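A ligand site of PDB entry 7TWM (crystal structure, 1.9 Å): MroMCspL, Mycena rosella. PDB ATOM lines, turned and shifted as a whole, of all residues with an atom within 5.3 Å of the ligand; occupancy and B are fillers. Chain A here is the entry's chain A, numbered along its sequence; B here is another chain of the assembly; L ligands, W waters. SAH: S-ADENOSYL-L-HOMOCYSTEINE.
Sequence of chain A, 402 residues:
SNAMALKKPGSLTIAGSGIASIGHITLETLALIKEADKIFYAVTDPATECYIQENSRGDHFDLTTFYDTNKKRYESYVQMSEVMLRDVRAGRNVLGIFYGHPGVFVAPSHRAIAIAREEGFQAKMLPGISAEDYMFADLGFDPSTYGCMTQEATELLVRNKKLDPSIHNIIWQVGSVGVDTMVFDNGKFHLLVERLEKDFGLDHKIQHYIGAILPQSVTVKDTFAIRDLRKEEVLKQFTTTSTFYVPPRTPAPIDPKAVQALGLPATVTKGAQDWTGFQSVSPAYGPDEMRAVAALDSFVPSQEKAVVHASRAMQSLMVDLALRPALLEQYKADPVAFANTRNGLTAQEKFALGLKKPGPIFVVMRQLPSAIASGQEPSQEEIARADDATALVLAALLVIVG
The side-chain carboxylate (OE2) of Glu 132 lies within hydrogen-bond range of the indole nitrogen (NE1) of Trp 172.
The backbone NH of His 101 is in hydrogen-bond range of the backbone carbonyl oxygen of Ile 129, 3.4 Å away.
The backbone NH (N) of Tyr 209 is in hydrogen-bond range of the backbone carbonyl oxygen (O) of Thr 243, 2.8 Å away.
The side-chain hydroxyl of Tyr 99 is in hydrogen-bond range of the backbone carbonyl oxygen of Ala 396 of chain B (2.7 Å).
O of Tyr 134 lies close to OH of Tyr 209, at 3.2 Å.
The side-chain hydroxyl (OG) of Ser 130 is in hydrogen-bond range of the backbone NH (N) of Glu 132.
The backbone carbonyl oxygen of Val 104 sits at hydrogen-bond distance from a nitrogen (N) of the ligand.
The backbone NH (N) of Gln 173 lies within hydrogen-bond range of an oxygen (O2') of the ligand.
NE2 of Gln 173 lies close to SD of the ligand (3.4 Å).
O2' of the ligand is in hydrogen-bond range of O of Ser 242 (3.1 Å).
O of Tyr 99 lies within hydrogen-bond range of N of the ligand (3.2 Å).
O of Thr 240 sits at hydrogen-bond distance from O3' of the ligand, at 2.7 Å.
N of Gly 211 sits at hydrogen-bond distance from N1 of the ligand, at 2.8 Å.
The backbone NH (N) of Ala 131 is in hydrogen-bond range of an oxygen (O) of the ligand (2.8 Å).
N of His 101 is in hydrogen-bond range of OXT of the ligand.
O of His 101 sits at hydrogen-bond distance from N of the ligand (2.9 Å).
OG1 of Thr 243 sits at hydrogen-bond distance from O2' of the ligand, at 2.7 Å.
The backbone carbonyl oxygen (O) of Gly 211 is in hydrogen-bond range of a nitrogen (N6) of the ligand (3.1 Å).
Water W1 lies within hydrogen-bond range of O of Tyr 99 (2.6 Å) and N of the ligand (2.9 Å).
Water W2 lies within hydrogen-bond range of the backbone carbonyl oxygen (O) of Ser 242 (2.7 Å), the backbone NH (N) of Val 174 (3.1 Å), the backbone carbonyl oxygen (O) of Thr 240 (3.4 Å) and an oxygen (O3') of the ligand (3.4 Å).
O of Phe 105 lies close to SD of the ligand (3.8 Å).
O of Thr 241 lies close to N3 of the ligand (3.0 Å).
Merely in contact with the ligand: Trp 172, MLE 398 of chain B, Ser 130, Ile 19, Ile 210, Tyr 209, Val 106, Gly 100, MLE 397 of chain B and Ile 213.
Hydrophobic or aromatic side chains within 4 Å of the ligand: Ile 19, Tyr 99, His 101, Val 104, Phe 105, Val 106, Ala 131, Trp 172, Tyr 209 and Ile 213.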
ATOM      1  N   ILE A  19      10.567 -25.268 -22.028  1.00  0.00           N
ATOM      2  CA  ILE A  19       9.831 -26.469 -21.624  1.00  0.00           C
ATOM      3  C   ILE A  19       9.197 -27.121 -22.846  1.00  0.00           C
ATOM      4  O   ILE A  19       9.280 -28.350 -22.995  1.00  0.00           O
ATOM      5  CB  ILE A  19       8.796 -26.177 -20.513  1.00  0.00           C
ATOM      6  CG1 ILE A  19       9.447 -25.516 -19.288  1.00  0.00           C
ATOM      7  CG2 ILE A  19       8.050 -27.466 -20.130  1.00  0.00           C
ATOM      8  CD1 ILE A  19      10.425 -26.417 -18.515  1.00  0.00           C
ATOM      9  N   TYR A  99      17.139 -27.991 -20.100  1.00  0.00           N
ATOM     10  CA  TYR A  99      15.758 -27.662 -20.388  1.00  0.00           C
ATOM     11  C   TYR A  99      15.256 -26.598 -19.414  1.00  0.00           C
ATOM     12  O   TYR A  99      15.764 -26.465 -18.292  1.00  0.00           O
ATOM     13  CB  TYR A  99      14.869 -28.896 -20.445  1.00  0.00           C
ATOM     14  CG  TYR A  99      14.558 -29.540 -19.124  1.00  0.00           C
ATOM     15  CD1 TYR A  99      13.366 -29.274 -18.468  1.00  0.00           C
ATOM     16  CD2 TYR A  99      15.431 -30.453 -18.547  1.00  0.00           C
ATOM     17  CE1 TYR A  99      13.065 -29.868 -17.251  1.00  0.00           C
ATOM     18  CE2 TYR A  99      15.150 -31.062 -17.332  1.00  0.00           C
ATOM     19  CZ  TYR A  99      13.947 -30.773 -16.694  1.00  0.00           C
ATOM     20  OH  TYR A  99      13.647 -31.381 -15.512  1.00  0.00           O
ATOM     21  N   GLY A 100      14.236 -25.854 -19.841  1.00  0.00           N
ATOM     22  CA  GLY A 100      13.671 -24.779 -19.044  1.00  0.00           C
ATOM     23  C   GLY A 100      14.631 -23.603 -18.970  1.00  0.00           C
ATOM     24  O   GLY A 100      15.262 -23.258 -19.964  1.00  0.00           O
ATOM     25  N   HIS A 101      14.703 -22.983 -17.780  1.00  0.00           N
ATOM     26  CA  HIS A 101      15.722 -22.017 -17.431  1.00  0.00           C
ATOM     27  C   HIS A 101      16.893 -22.793 -16.825  1.00  0.00           C
ATOM     28  O   HIS A 101      16.701 -23.584 -15.895  1.00  0.00           O
ATOM     29  CB  HIS A 101      15.116 -21.021 -16.431  1.00  0.00           C
ATOM     30  CG  HIS A 101      16.000 -19.871 -16.072  1.00  0.00           C
ATOM     31  ND1 HIS A 101      17.279 -20.040 -15.586  1.00  0.00           N
ATOM     32  CD2 HIS A 101      15.735 -18.542 -16.035  1.00  0.00           C
ATOM     33  CE1 HIS A 101      17.798 -18.860 -15.297  1.00  0.00           C
ATOM     34  NE2 HIS A 101      16.853 -17.923 -15.543  1.00  0.00           N
ATOM     35  N   PRO A 102      18.143 -22.598 -17.307  1.00  0.00           N
ATOM     36  CA  PRO A 102      19.260 -23.434 -16.855  1.00  0.00           C
ATOM     37  C   PRO A 102      19.763 -23.156 -15.431  1.00  0.00           C
ATOM     38  O   PRO A 102      20.644 -23.860 -14.944  1.00  0.00           O
ATOM     39  CB  PRO A 102      20.356 -23.053 -17.855  1.00  0.00           C
ATOM     40  CG  PRO A 102      20.048 -21.593 -18.176  1.00  0.00           C
ATOM     41  CD  PRO A 102      18.541 -21.558 -18.270  1.00  0.00           C
ATOM     42  N   VAL A 104      17.364 -22.627 -12.861  1.00  0.00           N
ATOM     43  CA  VAL A 104      16.193 -22.840 -12.012  1.00  0.00           C
ATOM     44  C   VAL A 104      16.067 -24.339 -11.744  1.00  0.00           C
ATOM     45  O   VAL A 104      15.771 -25.117 -12.647  1.00  0.00           O
ATOM     46  CB  VAL A 104      14.934 -22.221 -12.646  1.00  0.00           C
ATOM     47  CG1 VAL A 104      13.627 -22.602 -11.947  1.00  0.00           C
ATOM     48  CG2 VAL A 104      15.060 -20.712 -12.770  1.00  0.00           C
ATOM     49  N   PHE A 105      16.344 -24.726 -10.488  1.00  0.00           N
ATOM     50  CA  PHE A 105      16.353 -26.136 -10.113  1.00  0.00           C
ATOM     51  C   PHE A 105      17.401 -26.887 -10.941  1.00  0.00           C
ATOM     52  O   PHE A 105      17.159 -27.992 -11.415  1.00  0.00           O
ATOM     53  CB  PHE A 105      14.945 -26.750 -10.251  1.00  0.00           C
ATOM     54  CG  PHE A 105      13.939 -26.269  -9.225  1.00  0.00           C
ATOM     55  CD1 PHE A 105      13.408 -24.987  -9.284  1.00  0.00           C
ATOM     56  CD2 PHE A 105      13.548 -27.093  -8.173  1.00  0.00           C
ATOM     57  CE1 PHE A 105      12.502 -24.535  -8.325  1.00  0.00           C
ATOM     58  CE2 PHE A 105      12.642 -26.641  -7.214  1.00  0.00           C
ATOM     59  CZ  PHE A 105      12.136 -25.364  -7.284  1.00  0.00           C
ATOM     60  N   VAL A 106      18.584 -26.290 -11.113  1.00  0.00           N
ATOM     61  CA  VAL A 106      19.667 -26.957 -11.828  1.00  0.00           C
ATOM     62  C   VAL A 106      20.959 -26.738 -11.060  1.00  0.00           C
ATOM     63  O   VAL A 106      21.432 -25.604 -10.954  1.00  0.00           O
ATOM     64  CB  VAL A 106      19.814 -26.428 -13.280  1.00  0.00           C
ATOM     65  CG1 VAL A 106      20.958 -27.148 -14.008  1.00  0.00           C
ATOM     66  CG2 VAL A 106      18.531 -26.516 -14.095  1.00  0.00           C
ATOM     67  N   ILE A 129      12.999 -20.131 -20.609  1.00  0.00           N
ATOM     68  CA  ILE A 129      11.618 -20.214 -20.131  1.00  0.00           C
ATOM     69  C   ILE A 129      11.525 -21.326 -19.089  1.00  0.00           C
ATOM     70  O   ILE A 129      11.779 -22.474 -19.419  1.00  0.00           O
ATOM     71  CB  ILE A 129      10.680 -20.501 -21.338  1.00  0.00           C
ATOM     72  CG1 ILE A 129      10.754 -19.411 -22.417  1.00  0.00           C
ATOM     73  CG2 ILE A 129       9.245 -20.775 -20.857  1.00  0.00           C
ATOM     74  CD1 ILE A 129      10.159 -18.064 -22.018  1.00  0.00           C
ATOM     75  N   SER A 130      11.104 -20.993 -17.852  1.00  0.00           N
ATOM     76  CA  SER A 130      10.997 -21.990 -16.787  1.00  0.00           C
ATOM     77  C   SER A 130       9.607 -22.636 -16.753  1.00  0.00           C
ATOM     78  O   SER A 130       8.665 -22.161 -17.386  1.00  0.00           O
ATOM     79  CB  SER A 130      11.282 -21.367 -15.432  1.00  0.00           C
ATOM     80  OG  SER A 130      10.155 -20.607 -15.015  1.00  0.00           O
ATOM     81  N   ALA A 131       9.478 -23.706 -15.959  1.00  0.00           N
ATOM     82  CA  ALA A 131       8.169 -24.312 -15.727  1.00  0.00           C
ATOM     83  C   ALA A 131       7.195 -23.328 -15.076  1.00  0.00           C
ATOM     84  O   ALA A 131       5.997 -23.409 -15.309  1.00  0.00           O
ATOM     85  CB  ALA A 131       8.294 -25.589 -14.900  1.00  0.00           C
ATOM     86  N   GLU A 132       7.716 -22.423 -14.234  1.00  0.00           N
ATOM     87  CA  GLU A 132       6.892 -21.391 -13.620  1.00  0.00           C
ATOM     88  C   GLU A 132       6.357 -20.434 -14.679  1.00  0.00           C
ATOM     89  O   GLU A 132       5.178 -20.072 -14.641  1.00  0.00           O
ATOM     90  CB  GLU A 132       7.655 -20.624 -12.546  1.00  0.00           C
ATOM     91  CG  GLU A 132       7.244 -21.058 -11.154  1.00  0.00           C
ATOM     92  CD  GLU A 132       7.925 -20.348 -10.001  1.00  0.00           C
ATOM     93  OE1 GLU A 132       8.315 -19.159 -10.173  1.00  0.00           O
ATOM     94  OE2 GLU A 132       8.059 -20.993  -8.931  1.00  0.00           O
ATOM     95  N   TYR A 134       5.854 -21.107 -17.785  1.00  0.00           N
ATOM     96  CA  TYR A 134       4.855 -21.885 -18.516  1.00  0.00           C
ATOM     97  C   TYR A 134       3.552 -21.936 -17.696  1.00  0.00           C
ATOM     98  O   TYR A 134       2.461 -21.751 -18.239  1.00  0.00           O
ATOM     99  CB  TYR A 134       5.427 -23.280 -18.806  1.00  0.00           C
ATOM    100  CG  TYR A 134       4.922 -23.985 -20.045  1.00  0.00           C
ATOM    101  CD1 TYR A 134       4.028 -23.388 -20.926  1.00  0.00           C
ATOM    102  CD2 TYR A 134       5.382 -25.261 -20.350  1.00  0.00           C
ATOM    103  CE1 TYR A 134       3.608 -24.061 -22.075  1.00  0.00           C
ATOM    104  CE2 TYR A 134       4.990 -25.921 -21.496  1.00  0.00           C
ATOM    105  CZ  TYR A 134       4.073 -25.330 -22.352  1.00  0.00           C
ATOM    106  OH  TYR A 134       3.684 -26.002 -23.482  1.00  0.00           O
ATOM    107  N   ILE A 171       5.023 -25.541  -5.870  1.00  0.00           N
ATOM    108  CA  ILE A 171       5.852 -26.594  -5.294  1.00  0.00           C
ATOM    109  C   ILE A 171       6.339 -27.501  -6.415  1.00  0.00           C
ATOM    110  O   ILE A 171       5.537 -28.118  -7.114  1.00  0.00           O
ATOM    111  CB  ILE A 171       5.101 -27.381  -4.197  1.00  0.00           C
ATOM    112  CG1 ILE A 171       4.331 -26.449  -3.255  1.00  0.00           C
ATOM    113  CG2 ILE A 171       6.084 -28.281  -3.473  1.00  0.00           C
ATOM    114  CD1 ILE A 171       3.479 -27.175  -2.217  1.00  0.00           C
ATOM    115  N   TRP A 172       7.672 -27.585  -6.540  1.00  0.00           N
ATOM    116  CA  TRP A 172       8.302 -28.314  -7.618  1.00  0.00           C
ATOM    117  C   TRP A 172       8.786 -29.656  -7.092  1.00  0.00           C
ATOM    118  O   TRP A 172       8.992 -29.794  -5.893  1.00  0.00           O
ATOM    119  CB  TRP A 172       9.514 -27.529  -8.149  1.00  0.00           C
ATOM    120  CG  TRP A 172       9.269 -26.152  -8.667  1.00  0.00           C
ATOM    121  CD1 TRP A 172       8.618 -25.109  -8.047  1.00  0.00           C
ATOM    122  CD2 TRP A 172       9.742 -25.626  -9.921  1.00  0.00           C
ATOM    123  NE1 TRP A 172       8.657 -23.994  -8.839  1.00  0.00           N
ATOM    124  CE2 TRP A 172       9.353 -24.270  -9.986  1.00  0.00           C
ATOM    125  CE3 TRP A 172      10.448 -26.169 -10.998  1.00  0.00           C
ATOM    126  CZ2 TRP A 172       9.660 -23.445 -11.080  1.00  0.00           C
ATOM    127  CZ3 TRP A 172      10.739 -25.359 -12.086  1.00  0.00           C
ATOM    128  CH2 TRP A 172      10.338 -24.029 -12.129  1.00  0.00           C
ATOM    129  N   GLN A 173       9.013 -30.605  -8.022  1.00  0.00           N
ATOM    130  CA  GLN A 173       9.591 -31.921  -7.735  1.00  0.00           C
ATOM    131  C   GLN A 173       8.729 -32.670  -6.711  1.00  0.00           C
ATOM    132  O   GLN A 173       9.254 -33.374  -5.859  1.00  0.00           O
ATOM    133  CB  GLN A 173      11.078 -31.827  -7.348  1.00  0.00           C
ATOM    134  CG  GLN A 173      11.920 -31.099  -8.395  1.00  0.00           C
ATOM    135  CD  GLN A 173      13.386 -31.481  -8.412  1.00  0.00           C
ATOM    136  OE1 GLN A 173      13.999 -31.790  -7.388  1.00  0.00           O
ATOM    137  NE2 GLN A 173      13.974 -31.458  -9.598  1.00  0.00           N
ATOM    138  N   VAL A 174       7.395 -32.544  -6.843  1.00  0.00           N
ATOM    139  CA  VAL A 174       6.474 -33.172  -5.919  1.00  0.00           C
ATOM    140  C   VAL A 174       6.510 -34.689  -6.099  1.00  0.00           C
ATOM    141  O   VAL A 174       6.136 -35.420  -5.197  1.00  0.00           O
ATOM    142  CB  VAL A 174       5.034 -32.633  -6.021  1.00  0.00           C
ATOM    143  CG1 VAL A 174       4.972 -31.134  -5.737  1.00  0.00           C
ATOM    144  CG2 VAL A 174       4.384 -32.972  -7.356  1.00  0.00           C
ATOM    145  N   TYR A 209      -0.074 -29.318 -12.193  1.00  0.00           N
ATOM    146  CA  TYR A 209       0.326 -28.710 -13.459  1.00  0.00           C
ATOM    147  C   TYR A 209       1.424 -29.507 -14.145  1.00  0.00           C
ATOM    148  O   TYR A 209       2.461 -29.801 -13.542  1.00  0.00           O
ATOM    149  CB  TYR A 209       0.737 -27.237 -13.288  1.00  0.00           C
ATOM    150  CG  TYR A 209       1.277 -26.618 -14.555  1.00  0.00           C
ATOM    151  CD1 TYR A 209       0.471 -26.440 -15.677  1.00  0.00           C
ATOM    152  CD2 TYR A 209       2.605 -26.223 -14.640  1.00  0.00           C
ATOM    153  CE1 TYR A 209       0.959 -25.876 -16.845  1.00  0.00           C
ATOM    154  CE2 TYR A 209       3.115 -25.657 -15.812  1.00  0.00           C
ATOM    155  CZ  TYR A 209       2.289 -25.491 -16.901  1.00  0.00           C
ATOM    156  OH  TYR A 209       2.796 -24.928 -18.037  1.00  0.00           O
ATOM    157  N   ILE A 210       1.165 -29.863 -15.406  1.00  0.00           N
ATOM    158  CA  ILE A 210       2.181 -30.340 -16.344  1.00  0.00           C
ATOM    159  C   ILE A 210       1.998 -29.603 -17.662  1.00  0.00           C
ATOM    160  O   ILE A 210       1.002 -29.823 -18.374  1.00  0.00           O
ATOM    161  CB  ILE A 210       2.121 -31.878 -16.566  1.00  0.00           C
ATOM    162  CG1 ILE A 210       2.320 -32.665 -15.263  1.00  0.00           C
ATOM    163  CG2 ILE A 210       3.129 -32.284 -17.628  1.00  0.00           C
ATOM    164  CD1 ILE A 210       2.276 -34.178 -15.434  1.00  0.00           C
ATOM    165  N   GLY A 211       2.939 -28.708 -17.967  1.00  0.00           N
ATOM    166  CA  GLY A 211       2.924 -27.986 -19.234  1.00  0.00           C
ATOM    167  C   GLY A 211       3.259 -28.939 -20.390  1.00  0.00           C
ATOM    168  O   GLY A 211       4.028 -29.871 -20.188  1.00  0.00           O
ATOM    169  N   ALA A 212       2.660 -28.689 -21.571  1.00  0.00           N
ATOM    170  CA  ALA A 212       2.773 -29.557 -22.729  1.00  0.00           C
ATOM    171  C   ALA A 212       4.201 -29.532 -23.259  1.00  0.00           C
ATOM    172  O   ALA A 212       4.702 -28.476 -23.637  1.00  0.00           O
ATOM    173  CB  ALA A 212       1.801 -29.094 -23.812  1.00  0.00           C
ATOM    174  N   ILE A 213       4.844 -30.699 -23.292  1.00  0.00           N
ATOM    175  CA  ILE A 213       6.197 -30.772 -23.825  1.00  0.00           C
ATOM    176  C   ILE A 213       6.167 -30.916 -25.350  1.00  0.00           C
ATOM    177  O   ILE A 213       6.872 -30.195 -26.059  1.00  0.00           O
ATOM    178  CB  ILE A 213       6.982 -31.898 -23.141  1.00  0.00           C
ATOM    179  CG1 ILE A 213       7.222 -31.577 -21.664  1.00  0.00           C
ATOM    180  CG2 ILE A 213       8.292 -32.154 -23.880  1.00  0.00           C
ATOM    181  CD1 ILE A 213       7.592 -32.803 -20.845  1.00  0.00           C
ATOM    182  N   THR A 240       7.674 -37.120 -12.137  1.00  0.00           N
ATOM    183  CA  THR A 240       8.779 -36.201 -11.928  1.00  0.00           C
ATOM    184  C   THR A 240       8.604 -34.902 -12.716  1.00  0.00           C
ATOM    185  O   THR A 240       9.350 -33.938 -12.505  1.00  0.00           O
ATOM    186  CB  THR A 240      10.132 -36.877 -12.238  1.00  0.00           C
ATOM    187  OG1 THR A 240      10.160 -37.244 -13.609  1.00  0.00           O
ATOM    188  CG2 THR A 240      10.402 -38.075 -11.351  1.00  0.00           C
ATOM    189  N   THR A 241       7.603 -34.862 -13.604  1.00  0.00           N
ATOM    190  CA  THR A 241       7.292 -33.655 -14.376  1.00  0.00           C
ATOM    191  C   THR A 241       6.343 -32.726 -13.607  1.00  0.00           C
ATOM    192  O   THR A 241       6.192 -31.554 -13.968  1.00  0.00           O
ATOM    193  CB  THR A 241       6.660 -34.028 -15.726  1.00  0.00           C
ATOM    194  OG1 THR A 241       7.409 -35.107 -16.269  1.00  0.00           O
ATOM    195  CG2 THR A 241       6.673 -32.881 -16.713  1.00  0.00           C
ATOM    196  N   SER A 242       5.668 -33.261 -12.587  1.00  0.00           N
ATOM    197  CA  SER A 242       4.567 -32.570 -11.914  1.00  0.00           C
ATOM    198  C   SER A 242       5.066 -31.391 -11.074  1.00  0.00           C
ATOM    199  O   SER A 242       6.047 -31.514 -10.339  1.00  0.00           O
ATOM    200  CB  SER A 242       3.791 -33.527 -11.043  1.00  0.00           C
ATOM    201  OG  SER A 242       3.261 -34.595 -11.798  1.00  0.00           O
ATOM    202  N   THR A 243       4.303 -30.298 -11.139  1.00  0.00           N
ATOM    203  CA  THR A 243       4.395 -29.150 -10.241  1.00  0.00           C
ATOM    204  C   THR A 243       3.020 -28.886  -9.644  1.00  0.00           C
ATOM    205  O   THR A 243       2.006 -29.025 -10.345  1.00  0.00           O
ATOM    206  CB  THR A 243       4.886 -27.926 -11.034  1.00  0.00           C
ATOM    207  OG1 THR A 243       6.147 -28.257 -11.614  1.00  0.00           O
ATOM    208  CG2 THR A 243       5.027 -26.683 -10.179  1.00  0.00           C
ATOM    209  N   ALA B 396      14.423 -36.352 -15.864  1.00  0.00           N
ATOM    210  CA  ALA B 396      15.608 -35.527 -15.863  1.00  0.00           C
ATOM    211  C   ALA B 396      15.539 -34.548 -14.687  1.00  0.00           C
ATOM    212  O   ALA B 396      15.342 -33.346 -14.878  1.00  0.00           O
ATOM    213  CB  ALA B 396      15.794 -34.832 -17.195  1.00  0.00           C
ATOM    214  N   MLE B 397      15.745 -35.017 -13.435  1.00  0.00           N
ATOM    215  CN  MLE B 397      16.069 -36.412 -13.146  1.00  0.00           C
ATOM    216  CA  MLE B 397      15.783 -34.039 -12.320  1.00  0.00           C
ATOM    217  CB  MLE B 397      15.301 -34.568 -10.967  1.00  0.00           C
ATOM    218  CG  MLE B 397      13.857 -35.077 -10.947  1.00  0.00           C
ATOM    219  CD1 MLE B 397      13.452 -35.481  -9.535  1.00  0.00           C
ATOM    220  CD2 MLE B 397      12.890 -34.022 -11.503  1.00  0.00           C
ATOM    221  C   MLE B 397      17.198 -33.504 -12.203  1.00  0.00           C
ATOM    222  O   MLE B 397      18.161 -34.284 -12.286  1.00  0.00           O
ATOM    223  N   MLE B 398      17.391 -32.195 -12.059  1.00  0.00           N
ATOM    224  CN  MLE B 398      16.287 -31.239 -11.995  1.00  0.00           C
ATOM    225  CA  MLE B 398      18.770 -31.654 -12.042  1.00  0.00           C
ATOM    226  CB  MLE B 398      18.912 -30.682 -13.206  1.00  0.00           C
ATOM    227  CG  MLE B 398      19.102 -31.415 -14.523  1.00  0.00           C
ATOM    228  CD1 MLE B 398      18.467 -30.646 -15.666  1.00  0.00           C
ATOM    229  CD2 MLE B 398      20.584 -31.686 -14.764  1.00  0.00           C
ATOM    230  C   MLE B 398      19.205 -30.980 -10.747  1.00  0.00           C
ATOM    231  O   MLE B 398      20.223 -30.271 -10.741  1.00  0.00           O
HETATM  232  N   SAH L   1      15.192 -25.960 -15.159  1.00  0.00           N
HETATM  233  CA  SAH L   1      13.776 -26.414 -15.220  1.00  0.00           C
HETATM  234  CB  SAH L   1      13.366 -27.143 -13.936  1.00  0.00           C
HETATM  235  CG  SAH L   1      14.167 -28.410 -13.653  1.00  0.00           C
HETATM  236  SD  SAH L   1      13.682 -29.274 -12.124  1.00  0.00           S
HETATM  237  C   SAH L   1      12.878 -25.181 -15.393  1.00  0.00           C
HETATM  238  O   SAH L   1      11.651 -25.339 -15.350  1.00  0.00           O
HETATM  239  OXT SAH L   1      13.323 -24.033 -15.581  1.00  0.00           O
HETATM  240  C5' SAH L   1      12.296 -30.318 -12.655  1.00  0.00           C
HETATM  241  C4' SAH L   1      11.011 -29.833 -12.036  1.00  0.00           C
HETATM  242  O4' SAH L   1      10.498 -28.732 -12.824  1.00  0.00           O
HETATM  243  C3' SAH L   1       9.882 -30.863 -12.044  1.00  0.00           C
HETATM  244  O3' SAH L   1       9.979 -31.796 -10.981  1.00  0.00           O
HETATM  245  C2' SAH L   1       8.657 -29.951 -11.995  1.00  0.00           C
HETATM  246  O2' SAH L   1       8.387 -29.459 -10.705  1.00  0.00           O
HETATM  247  C1' SAH L   1       9.102 -28.848 -12.949  1.00  0.00           C
HETATM  248  N9  SAH L   1       8.756 -29.133 -14.339  1.00  0.00           N
HETATM  249  C8  SAH L   1       9.562 -29.629 -15.318  1.00  0.00           C
HETATM  250  N7  SAH L   1       8.948 -29.838 -16.457  1.00  0.00           N
HETATM  251  C5  SAH L   1       7.641 -29.450 -16.199  1.00  0.00           C
HETATM  252  C6  SAH L   1       6.481 -29.424 -17.012  1.00  0.00           C
HETATM  253  N6  SAH L   1       6.468 -29.848 -18.276  1.00  0.00           N
HETATM  254  N1  SAH L   1       5.328 -28.990 -16.445  1.00  0.00           N
HETATM  255  C2  SAH L   1       5.359 -28.586 -15.161  1.00  0.00           C
HETATM  256  N3  SAH L   1       6.374 -28.578 -14.303  1.00  0.00           N
HETATM  257  C4  SAH L   1       7.510 -29.016 -14.894  1.00  0.00           C
HETATM  258  O   HOH W   1      16.630 -28.093 -16.488  1.00  0.00           O
HETATM  259  O   HOH W   2       7.529 -33.734  -9.686  1.00  0.00           O
HETATM  260  O   HOH W   3       9.301 -30.891 -18.968  1.00  0.00           O
